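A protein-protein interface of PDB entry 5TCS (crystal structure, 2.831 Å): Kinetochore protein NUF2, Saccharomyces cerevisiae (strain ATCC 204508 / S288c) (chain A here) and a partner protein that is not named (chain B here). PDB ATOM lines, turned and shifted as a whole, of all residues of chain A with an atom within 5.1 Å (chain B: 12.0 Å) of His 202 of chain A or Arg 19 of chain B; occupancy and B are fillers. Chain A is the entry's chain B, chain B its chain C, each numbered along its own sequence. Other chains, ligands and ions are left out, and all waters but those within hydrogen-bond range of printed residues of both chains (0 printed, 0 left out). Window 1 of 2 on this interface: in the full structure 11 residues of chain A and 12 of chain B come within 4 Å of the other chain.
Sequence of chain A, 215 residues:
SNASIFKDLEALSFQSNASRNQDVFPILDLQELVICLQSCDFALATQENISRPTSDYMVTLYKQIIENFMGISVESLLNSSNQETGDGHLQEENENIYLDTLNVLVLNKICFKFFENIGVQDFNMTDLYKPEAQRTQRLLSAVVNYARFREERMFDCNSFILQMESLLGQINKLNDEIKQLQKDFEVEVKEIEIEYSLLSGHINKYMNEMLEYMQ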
ATOM      1  N   GLU A 195     -13.983  12.581 -13.153  1.00  0.00           N
ATOM      2  CA  GLU A 195     -15.248  12.089 -13.688  1.00  0.00           C
ATOM      3  C   GLU A 195     -16.403  12.990 -13.276  1.00  0.00           C
ATOM      4  O   GLU A 195     -17.248  13.351 -14.103  1.00  0.00           O
ATOM      5  CB  GLU A 195     -15.502  10.652 -13.235  1.00  0.00           C
ATOM      6  CG  GLU A 195     -14.925   9.597 -14.164  1.00  0.00           C
ATOM      7  CD  GLU A 195     -15.468   9.688 -15.580  1.00  0.00           C
ATOM      8  OE1 GLU A 195     -16.598  10.189 -15.752  1.00  0.00           O
ATOM      9  OE2 GLU A 195     -14.764   9.258 -16.521  1.00  0.00           O
ATOM     10  N   SER A 197     -16.331  16.102 -12.657  1.00  0.00           N
ATOM     11  CA  SER A 197     -16.280  17.313 -13.470  1.00  0.00           C
ATOM     12  C   SER A 197     -16.887  17.070 -14.846  1.00  0.00           C
ATOM     13  O   SER A 197     -17.655  17.900 -15.351  1.00  0.00           O
ATOM     14  CB  SER A 197     -14.842  17.811 -13.597  1.00  0.00           C
ATOM     15  OG  SER A 197     -14.061  16.910 -14.357  1.00  0.00           O
ATOM     16  N   LEU A 198     -16.556  15.935 -15.470  1.00  0.00           N
ATOM     17  CA  LEU A 198     -17.163  15.610 -16.757  1.00  0.00           C
ATOM     18  C   LEU A 198     -18.682  15.512 -16.644  1.00  0.00           C
ATOM     19  O   LEU A 198     -19.409  15.953 -17.543  1.00  0.00           O
ATOM     20  CB  LEU A 198     -16.583  14.303 -17.298  1.00  0.00           C
ATOM     21  CG  LEU A 198     -15.103  14.310 -17.699  1.00  0.00           C
ATOM     22  CD1 LEU A 198     -14.734  12.987 -18.356  1.00  0.00           C
ATOM     23  CD2 LEU A 198     -14.776  15.473 -18.629  1.00  0.00           C
ATOM     24  N   LEU A 199     -19.179  14.941 -15.546  1.00  0.00           N
ATOM     25  CA  LEU A 199     -20.621  14.809 -15.362  1.00  0.00           C
ATOM     26  C   LEU A 199     -21.280  16.169 -15.177  1.00  0.00           C
ATOM     27  O   LEU A 199     -22.354  16.425 -15.729  1.00  0.00           O
ATOM     28  CB  LEU A 199     -20.913  13.905 -14.164  1.00  0.00           C
ATOM     29  CG  LEU A 199     -22.387  13.718 -13.796  1.00  0.00           C
ATOM     30  CD1 LEU A 199     -23.176  13.176 -14.973  1.00  0.00           C
ATOM     31  CD2 LEU A 199     -22.515  12.798 -12.595  1.00  0.00           C
ATOM     32  N   SER A 200     -20.656  17.050 -14.394  1.00  0.00           N
ATOM     33  CA  SER A 200     -21.184  18.396 -14.206  1.00  0.00           C
ATOM     34  C   SER A 200     -21.243  19.143 -15.530  1.00  0.00           C
ATOM     35  O   SER A 200     -22.287  19.692 -15.899  1.00  0.00           O
ATOM     36  CB  SER A 200     -20.325  19.160 -13.196  1.00  0.00           C
ATOM     37  OG  SER A 200     -20.658  20.539 -13.178  1.00  0.00           O
ATOM     38  N   GLY A 201     -20.127  19.180 -16.258  1.00  0.00           N
ATOM     39  CA  GLY A 201     -20.143  19.794 -17.575  1.00  0.00           C
ATOM     40  C   GLY A 201     -21.216  19.207 -18.468  1.00  0.00           C
ATOM     41  O   GLY A 201     -21.882  19.927 -19.216  1.00  0.00           O
ATOM     42  N   HIS A 202     -21.409  17.888 -18.391  1.00  0.00           N
ATOM     43  CA  HIS A 202     -22.441  17.234 -19.186  1.00  0.00           C
ATOM     44  C   HIS A 202     -23.826  17.759 -18.828  1.00  0.00           C
ATOM     45  O   HIS A 202     -24.599  18.156 -19.706  1.00  0.00           O
ATOM     46  CB  HIS A 202     -22.368  15.722 -18.978  1.00  0.00           C
ATOM     47  CG  HIS A 202     -23.132  14.935 -19.997  1.00  0.00           C
ATOM     48  ND1 HIS A 202     -22.695  14.775 -21.294  1.00  0.00           N
ATOM     49  CD2 HIS A 202     -24.305  14.265 -19.910  1.00  0.00           C
ATOM     50  CE1 HIS A 202     -23.565  14.038 -21.962  1.00  0.00           C
ATOM     51  NE2 HIS A 202     -24.552  13.716 -21.145  1.00  0.00           N
ATOM     52  N   ILE A 203     -24.156  17.768 -17.535  1.00  0.00           N
ATOM     53  CA  ILE A 203     -25.480  18.204 -17.095  1.00  0.00           C
ATOM     54  C   ILE A 203     -25.709  19.666 -17.460  1.00  0.00           C
ATOM     55  O   ILE A 203     -26.760  20.031 -17.999  1.00  0.00           O
ATOM     56  CB  ILE A 203     -25.639  17.958 -15.582  1.00  0.00           C
ATOM     57  CG1 ILE A 203     -25.930  16.476 -15.328  1.00  0.00           C
ATOM     58  CG2 ILE A 203     -26.746  18.831 -14.984  1.00  0.00           C
ATOM     59  CD1 ILE A 203     -25.701  16.034 -13.895  1.00  0.00           C
ATOM     60  N   ASN A 204     -24.737  20.529 -17.156  1.00  0.00           N
ATOM     61  CA  ASN A 204     -24.861  21.940 -17.513  1.00  0.00           C
ATOM     62  C   ASN A 204     -25.097  22.104 -19.008  1.00  0.00           C
ATOM     63  O   ASN A 204     -25.955  22.887 -19.431  1.00  0.00           O
ATOM     64  CB  ASN A 204     -23.610  22.705 -17.081  1.00  0.00           C
ATOM     65  CG  ASN A 204     -23.655  23.125 -15.626  1.00  0.00           C
ATOM     66  OD1 ASN A 204     -24.462  23.971 -15.238  1.00  0.00           O
ATOM     67  ND2 ASN A 204     -22.780  22.543 -14.814  1.00  0.00           N
ATOM     68  N   LYS A 205     -24.331  21.380 -19.825  1.00  0.00           N
ATOM     69  CA  LYS A 205     -24.556  21.385 -21.267  1.00  0.00           C
ATOM     70  C   LYS A 205     -25.994  21.003 -21.590  1.00  0.00           C
ATOM     71  O   LYS A 205     -26.664  21.654 -22.401  1.00  0.00           O
ATOM     72  CB  LYS A 205     -23.575  20.418 -21.931  1.00  0.00           C
ATOM     73  CG  LYS A 205     -23.567  20.439 -23.444  1.00  0.00           C
ATOM     74  CD  LYS A 205     -22.607  19.386 -23.975  1.00  0.00           C
ATOM     75  CE  LYS A 205     -22.854  19.077 -25.439  1.00  0.00           C
ATOM     76  NZ  LYS A 205     -22.029  17.925 -25.901  1.00  0.00           N
ATOM     77  N   TYR A 206     -26.482  19.938 -20.952  1.00  0.00           N
ATOM     78  CA  TYR A 206     -27.852  19.484 -21.158  1.00  0.00           C
ATOM     79  C   TYR A 206     -28.858  20.589 -20.857  1.00  0.00           C
ATOM     80  O   TYR A 206     -29.809  20.794 -21.618  1.00  0.00           O
ATOM     81  CB  TYR A 206     -28.102  18.258 -20.280  1.00  0.00           C
ATOM     82  CG  TYR A 206     -29.545  17.840 -20.132  1.00  0.00           C
ATOM     83  CD1 TYR A 206     -30.199  17.154 -21.144  1.00  0.00           C
ATOM     84  CD2 TYR A 206     -30.242  18.104 -18.963  1.00  0.00           C
ATOM     85  CE1 TYR A 206     -31.508  16.760 -21.005  1.00  0.00           C
ATOM     86  CE2 TYR A 206     -31.552  17.715 -18.812  1.00  0.00           C
ATOM     87  CZ  TYR A 206     -32.180  17.042 -19.836  1.00  0.00           C
ATOM     88  OH  TYR A 206     -33.490  16.647 -19.693  1.00  0.00           O
ATOM     89  N   ASN B  10     -16.106   0.505  -7.712  1.00  0.00           N
ATOM     90  CA  ASN B  10     -15.321   1.391  -8.570  1.00  0.00           C
ATOM     91  C   ASN B  10     -16.152   2.639  -8.829  1.00  0.00           C
ATOM     92  O   ASN B  10     -17.046   2.634  -9.692  1.00  0.00           O
ATOM     93  CB  ASN B  10     -14.914   0.723  -9.881  1.00  0.00           C
ATOM     94  CG  ASN B  10     -13.955   1.578 -10.692  1.00  0.00           C
ATOM     95  OD1 ASN B  10     -13.581   2.676 -10.275  1.00  0.00           O
ATOM     96  ND2 ASN B  10     -13.540   1.074 -11.846  1.00  0.00           N
ATOM     97  N   PRO B  11     -15.878   3.738  -8.120  1.00  0.00           N
ATOM     98  CA  PRO B  11     -16.744   4.923  -8.272  1.00  0.00           C
ATOM     99  C   PRO B  11     -16.543   5.656  -9.583  1.00  0.00           C
ATOM    100  O   PRO B  11     -17.526   6.124 -10.179  1.00  0.00           O
ATOM    101  CB  PRO B  11     -16.350   5.786  -7.066  1.00  0.00           C
ATOM    102  CG  PRO B  11     -14.921   5.422  -6.809  1.00  0.00           C
ATOM    103  CD  PRO B  11     -14.791   3.965  -7.152  1.00  0.00           C
ATOM    104  N   VAL B  12     -15.301   5.783 -10.051  1.00  0.00           N
ATOM    105  CA  VAL B  12     -15.041   6.425 -11.339  1.00  0.00           C
ATOM    106  C   VAL B  12     -15.926   5.812 -12.417  1.00  0.00           C
ATOM    107  O   VAL B  12     -16.644   6.516 -13.142  1.00  0.00           O
ATOM    108  CB  VAL B  12     -13.545   6.303 -11.695  1.00  0.00           C
ATOM    109  CG1 VAL B  12     -13.246   6.915 -13.053  1.00  0.00           C
ATOM    110  CG2 VAL B  12     -12.693   6.977 -10.629  1.00  0.00           C
ATOM    111  N   GLU B  13     -15.888   4.485 -12.531  1.00  0.00           N
ATOM    112  CA  GLU B  13     -16.683   3.795 -13.539  1.00  0.00           C
ATOM    113  C   GLU B  13     -18.174   4.036 -13.341  1.00  0.00           C
ATOM    114  O   GLU B  13     -18.935   4.034 -14.316  1.00  0.00           O
ATOM    115  CB  GLU B  13     -16.365   2.300 -13.501  1.00  0.00           C
ATOM    116  CG  GLU B  13     -17.128   1.468 -14.519  1.00  0.00           C
ATOM    117  CD  GLU B  13     -18.293   0.713 -13.910  1.00  0.00           C
ATOM    118  OE1 GLU B  13     -18.193   0.299 -12.735  1.00  0.00           O
ATOM    119  OE2 GLU B  13     -19.312   0.530 -14.609  1.00  0.00           O
ATOM    120  N   PHE B  14     -18.616   4.245 -12.098  1.00  0.00           N
ATOM    121  CA  PHE B  14     -20.026   4.536 -11.861  1.00  0.00           C
ATOM    122  C   PHE B  14     -20.396   5.915 -12.394  1.00  0.00           C
ATOM    123  O   PHE B  14     -21.375   6.062 -13.134  1.00  0.00           O
ATOM    124  CB  PHE B  14     -20.353   4.430 -10.369  1.00  0.00           C
ATOM    125  CG  PHE B  14     -20.535   3.019  -9.880  1.00  0.00           C
ATOM    126  CD1 PHE B  14     -21.483   2.188 -10.454  1.00  0.00           C
ATOM    127  CD2 PHE B  14     -19.775   2.533  -8.829  1.00  0.00           C
ATOM    128  CE1 PHE B  14     -21.656   0.893 -10.004  1.00  0.00           C
ATOM    129  CE2 PHE B  14     -19.943   1.237  -8.374  1.00  0.00           C
ATOM    130  CZ  PHE B  14     -20.886   0.418  -8.962  1.00  0.00           C
ATOM    131  N   LEU B  15     -19.626   6.943 -12.026  1.00  0.00           N
ATOM    132  CA  LEU B  15     -19.897   8.282 -12.540  1.00  0.00           C
ATOM    133  C   LEU B  15     -19.885   8.293 -14.063  1.00  0.00           C
ATOM    134  O   LEU B  15     -20.780   8.862 -14.699  1.00  0.00           O
ATOM    135  CB  LEU B  15     -18.873   9.279 -11.993  1.00  0.00           C
ATOM    136  CG  LEU B  15     -18.959   9.672 -10.516  1.00  0.00           C
ATOM    137  CD1 LEU B  15     -17.913  10.732 -10.214  1.00  0.00           C
ATOM    138  CD2 LEU B  15     -20.342  10.178 -10.140  1.00  0.00           C
ATOM    139  N   LYS B  16     -18.871   7.670 -14.667  1.00  0.00           N
ATOM    140  CA  LYS B  16     -18.830   7.562 -16.122  1.00  0.00           C
ATOM    141  C   LYS B  16     -20.094   6.895 -16.652  1.00  0.00           C
ATOM    142  O   LYS B  16     -20.721   7.383 -17.602  1.00  0.00           O
ATOM    143  CB  LYS B  16     -17.584   6.783 -16.540  1.00  0.00           C
ATOM    144  CG  LYS B  16     -17.420   6.587 -18.039  1.00  0.00           C
ATOM    145  CD  LYS B  16     -16.191   5.740 -18.337  1.00  0.00           C
ATOM    146  CE  LYS B  16     -15.979   5.556 -19.830  1.00  0.00           C
ATOM    147  NZ  LYS B  16     -14.758   4.757 -20.124  1.00  0.00           N
ATOM    148  N   GLU B  17     -20.490   5.777 -16.038  1.00  0.00           N
ATOM    149  CA  GLU B  17     -21.671   5.049 -16.488  1.00  0.00           C
ATOM    150  C   GLU B  17     -22.931   5.896 -16.363  1.00  0.00           C
ATOM    151  O   GLU B  17     -23.902   5.674 -17.096  1.00  0.00           O
ATOM    152  CB  GLU B  17     -21.813   3.754 -15.688  1.00  0.00           C
ATOM    153  CG  GLU B  17     -22.838   2.778 -16.241  1.00  0.00           C
ATOM    154  CD  GLU B  17     -22.834   1.450 -15.504  1.00  0.00           C
ATOM    155  OE1 GLU B  17     -21.780   1.081 -14.944  1.00  0.00           O
ATOM    156  OE2 GLU B  17     -23.885   0.776 -15.481  1.00  0.00           O
ATOM    157  N   VAL B  18     -22.941   6.864 -15.445  1.00  0.00           N
ATOM    158  CA  VAL B  18     -24.075   7.772 -15.335  1.00  0.00           C
ATOM    159  C   VAL B  18     -24.011   8.840 -16.418  1.00  0.00           C
ATOM    160  O   VAL B  18     -25.039   9.230 -16.982  1.00  0.00           O
ATOM    161  CB  VAL B  18     -24.122   8.396 -13.927  1.00  0.00           C
ATOM    162  CG1 VAL B  18     -25.191   9.486 -13.848  1.00  0.00           C
ATOM    163  CG2 VAL B  18     -24.388   7.323 -12.885  1.00  0.00           C
ATOM    164  N   ARG B  19     -22.809   9.330 -16.725  1.00  0.00           N
ATOM    165  CA  ARG B  19     -22.673  10.345 -17.764  1.00  0.00           C
ATOM    166  C   ARG B  19     -23.093   9.797 -19.122  1.00  0.00           C
ATOM    167  O   ARG B  19     -23.800  10.472 -19.882  1.00  0.00           O
ATOM    168  CB  ARG B  19     -21.233  10.855 -17.819  1.00  0.00           C
ATOM    169  CG  ARG B  19     -21.058  12.102 -18.675  1.00  0.00           C
ATOM    170  CD  ARG B  19     -19.596  12.440 -18.909  1.00  0.00           C
ATOM    171  NE  ARG B  19     -18.960  11.507 -19.842  1.00  0.00           N
ATOM    172  CZ  ARG B  19     -18.015  10.622 -19.530  1.00  0.00           C
ATOM    173  NH1 ARG B  19     -17.548  10.521 -18.290  1.00  0.00           N
ATOM    174  NH2 ARG B  19     -17.521   9.832 -20.474  1.00  0.00           N
ATOM    175  N   GLU B  20     -22.668   8.574 -19.446  1.00  0.00           N
ATOM    176  CA  GLU B  20     -22.973   8.013 -20.758  1.00  0.00           C
ATOM    177  C   GLU B  20     -24.461   7.726 -20.923  1.00  0.00           C
ATOM    178  O   GLU B  20     -24.982   7.797 -22.042  1.00  0.00           O
ATOM    179  CB  GLU B  20     -22.153   6.743 -20.982  1.00  0.00           C
ATOM    180  CG  GLU B  20     -20.657   7.000 -21.105  1.00  0.00           C
ATOM    181  CD  GLU B  20     -19.843   5.721 -21.159  1.00  0.00           C
ATOM    182  OE1 GLU B  20     -20.412   4.639 -20.901  1.00  0.00           O
ATOM    183  OE2 GLU B  20     -18.634   5.799 -21.463  1.00  0.00           O
ATOM    184  N   SER B  21     -25.158   7.405 -19.835  1.00  0.00           N
ATOM    185  CA  SER B  21     -26.593   7.146 -19.886  1.00  0.00           C
ATOM    186  C   SER B  21     -27.428   8.421 -19.884  1.00  0.00           C
ATOM    187  O   SER B  21     -28.657   8.336 -19.971  1.00  0.00           O
ATOM    188  CB  SER B  21     -27.006   6.267 -18.701  1.00  0.00           C
ATOM    189  OG  SER B  21     -26.409   4.985 -18.784  1.00  0.00           O
ATOM    190  N   PHE B  22     -26.794   9.590 -19.794  1.00  0.00           N
ATOM    191  CA  PHE B  22     -27.498  10.869 -19.713  1.00  0.00           C
ATOM    192  C   PHE B  22     -27.731  11.374 -21.135  1.00  0.00           C
ATOM    193  O   PHE B  22     -27.000  12.213 -21.666  1.00  0.00           O
ATOM    194  CB  PHE B  22     -26.690  11.854 -18.880  1.00  0.00           C
ATOM    195  CG  PHE B  22     -27.516  12.889 -18.175  1.00  0.00           C
ATOM    196  CD1 PHE B  22     -28.041  12.633 -16.920  1.00  0.00           C
ATOM    197  CD2 PHE B  22     -27.748  14.124 -18.754  1.00  0.00           C
ATOM    198  CE1 PHE B  22     -28.793  13.585 -16.261  1.00  0.00           C
ATOM    199  CE2 PHE B  22     -28.498  15.080 -18.099  1.00  0.00           C
ATOM    200  CZ  PHE B  22     -29.021  14.810 -16.850  1.00  0.00           C
ATOM    201  N   ASP B  23     -28.780  10.844 -21.763  1.00  0.00           N
ATOM    202  CA  ASP B  23     -29.037  11.098 -23.178  1.00  0.00           C
ATOM    203  C   ASP B  23     -29.573  12.513 -23.363  1.00  0.00           C
ATOM    204  O   ASP B  23     -30.717  12.805 -23.001  1.00  0.00           O
ATOM    205  CB  ASP B  23     -30.017  10.065 -23.724  1.00  0.00           C
ATOM    206  CG  ASP B  23     -29.900   9.887 -25.225  1.00  0.00           C
ATOM    207  OD1 ASP B  23     -29.494  10.849 -25.909  1.00  0.00           O
ATOM    208  OD2 ASP B  23     -30.209   8.782 -25.720  1.00  0.00           O
ATOM    209  N   ILE B  24     -28.750  13.389 -23.937  1.00  0.00           N
ATOM    210  CA  ILE B  24     -29.148  14.778 -24.156  1.00  0.00           C
ATOM    211  C   ILE B  24     -29.980  14.907 -25.426  1.00  0.00           C
ATOM    212  O   ILE B  24     -31.100  15.435 -25.415  1.00  0.00           O
ATOM    213  CB  ILE B  24     -27.901  15.683 -24.210  1.00  0.00           C
ATOM    214  CG1 ILE B  24     -27.242  15.749 -22.829  1.00  0.00           C
ATOM    215  CG2 ILE B  24     -28.260  17.081 -24.737  1.00  0.00           C
ATOM    216  CD1 ILE B  24     -26.050  16.692 -22.734  1.00  0.00           C
ATOM    217  N   GLN B  25     -29.430  14.435 -26.548  1.00  0.00           N
ATOM    218  CA  GLN B  25     -30.092  14.617 -27.833  1.00  0.00           C
ATOM    219  C   GLN B  25     -31.481  13.998 -27.838  1.00  0.00           C
ATOM    220  O   GLN B  25     -32.347  14.425 -28.609  1.00  0.00           O
ATOM    221  CB  GLN B  25     -29.242  14.014 -28.951  1.00  0.00           C
ATOM    222  CG  GLN B  25     -29.605  14.522 -30.337  1.00  0.00           C
ATOM    223  CD  GLN B  25     -29.284  15.994 -30.516  1.00  0.00           C
ATOM    224  OE1 GLN B  25     -28.160  16.430 -30.260  1.00  0.00           O
ATOM    225  NE2 GLN B  25     -30.273  16.771 -30.947  1.00  0.00           N
ATOM    226  N   GLN B  26     -31.716  12.993 -26.995  1.00  0.00           N
ATOM    227  CA  GLN B  26     -33.040  12.388 -26.919  1.00  0.00           C
ATOM    228  C   GLN B  26     -34.068  13.394 -26.412  1.00  0.00           C
ATOM    229  O   GLN B  26     -35.105  13.618 -27.049  1.00  0.00           O
ATOM    230  CB  GLN B  26     -32.995  11.155 -26.018  1.00  0.00           C
ATOM    231  CG  GLN B  26     -34.316  10.419 -25.907  1.00  0.00           C
ATOM    232  CD  GLN B  26     -34.182   9.112 -25.154  1.00  0.00           C
ATOM    233  OE1 GLN B  26     -33.550   8.170 -25.632  1.00  0.00           O
ATOM    234  NE2 GLN B  26     -34.770   9.052 -23.965  1.00  0.00           N
ATOM    235  N   ASP B  27     -33.789  14.019 -25.268  1.00  0.00           N
ATOM    236  CA  ASP B  27     -34.721  14.996 -24.715  1.00  0.00           C
ATOM    237  C   ASP B  27     -34.805  16.239 -25.590  1.00  0.00           C
ATOM    238  O   ASP B  27     -35.882  16.830 -25.730  1.00  0.00           O
ATOM    239  CB  ASP B  27     -34.310  15.370 -23.293  1.00  0.00           C
ATOM    240  CG  ASP B  27     -34.542  14.245 -22.310  1.00  0.00           C
ATOM    241  OD1 ASP B  27     -35.142  13.222 -22.700  1.00  0.00           O
ATOM    242  OD2 ASP B  27     -34.129  14.387 -21.142  1.00  0.00           O
ATOM    243  N   VAL B  28     -33.686  16.664 -26.178  1.00  0.00           N
ATOM    244  CA  VAL B  28     -33.738  17.787 -27.112  1.00  0.00           C
ATOM    245  C   VAL B  28     -34.698  17.472 -28.254  1.00  0.00           C
ATOM    246  O   VAL B  28     -35.611  18.251 -28.560  1.00  0.00           O
ATOM    247  CB  VAL B  28     -32.326  18.122 -27.628  1.00  0.00           C
ATOM    248  CG1 VAL B  28     -32.391  19.008 -28.870  1.00  0.00           C
ATOM    249  CG2 VAL B  28     -31.525  18.809 -26.539  1.00  0.00           C
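Of chain B, only Arg 19 (3.6 Å), Phe 22 (2.9 Å) and Ile 24 (3.7 Å) come within 4 Å of His 202 of chain A. Of chain B, only Val 12, Leu 15, Lys 16 and Arg 19 come within 4 Å of Glu 195 of chain A. No residue of chain B comes within 4 Å of Ser 200 of chain A. No residue of chain B comes within 4 Å of Gly 201 of chain A. No residue of chain B comes within 4 Å of Lys 205 of chain A. Printed residues of chain B within 4 Å of Tyr 206 of chain A: Phe 22 (3.6 Å), Ile 24 (3.6 Å) and Asp 27 (2.8 Å). Printed residues of chain A within 4 Å of Lys 16 of chain B: Glu 195. Of the printed residues of chain A, Leu 15 of chain B touches Glu 195. Printed residues of chain A within 4 Å of Phe 22 of chain B: His 202 (2.9 Å), Ile 203 (3.8 Å) and Tyr 206 (3.6 Å). Ser 197 of chain A touches none of the printed residues of chain B. The nearest residue of chain B that does not touch His 202 of chain A is Asp 23 of chain B (5.1 Å). The nearest printed residue of chain A that does not touch Asp 27 of chain B is His 202 of chain A (9.6 Å).
Among the printed residues, pairs that only touch across the chains: Glu 195 of chain A with Val 12 of chain B, Glu 195 of chain A with Lys 16 of chain B, His 202 of chain A with Arg 19 of chain B, Tyr 206 of chain A with Ile 24 of chain B, Tyr 206 of chain A with Phe 22 of chain B, His 202 of chain A with Ile 24 of chain B, Leu 198 of chain A with Arg 19 of chain B, Ile 203 of chain A with Phe 22 of chain B and Glu 195 of chain A with Leu 15 of chain B.
Of the 19 printed residues of chain B, 7 touch a printed residue of chain A. Hydrophobic or aromatic side chains of chain B within 4 Å of the printed part of chain A: Val 12, Leu 15, Phe 22 and Ile 24. Along chain B the printed residues that touch a printed residue of chain A span positions 12 to 27. Of the 11 printed residues of chain A, 5 touch a printed residue of chain B. Hydrophobic or aromatic side chains of chain A within 4 Å of the printed part of chain B: Leu 198, His 202, Ile 203 and Tyr 206.
The side-chain carboxylate (OE1) of Glu 195 of chain A is in salt-bridge range of the guanidinium group (NH1) of Arg 19 of chain B, 2.7 Å away. The backbone carbonyl oxygen (O) of Phe 22 of chain B is in hydrogen-bond range of a ring nitrogen (NE2) of His 202 of chain A (2.9 Å). OH of Tyr 206 of chain A sits at hydrogen-bond distance from OD2 of Asp 27 of chain B (2.8 Å).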
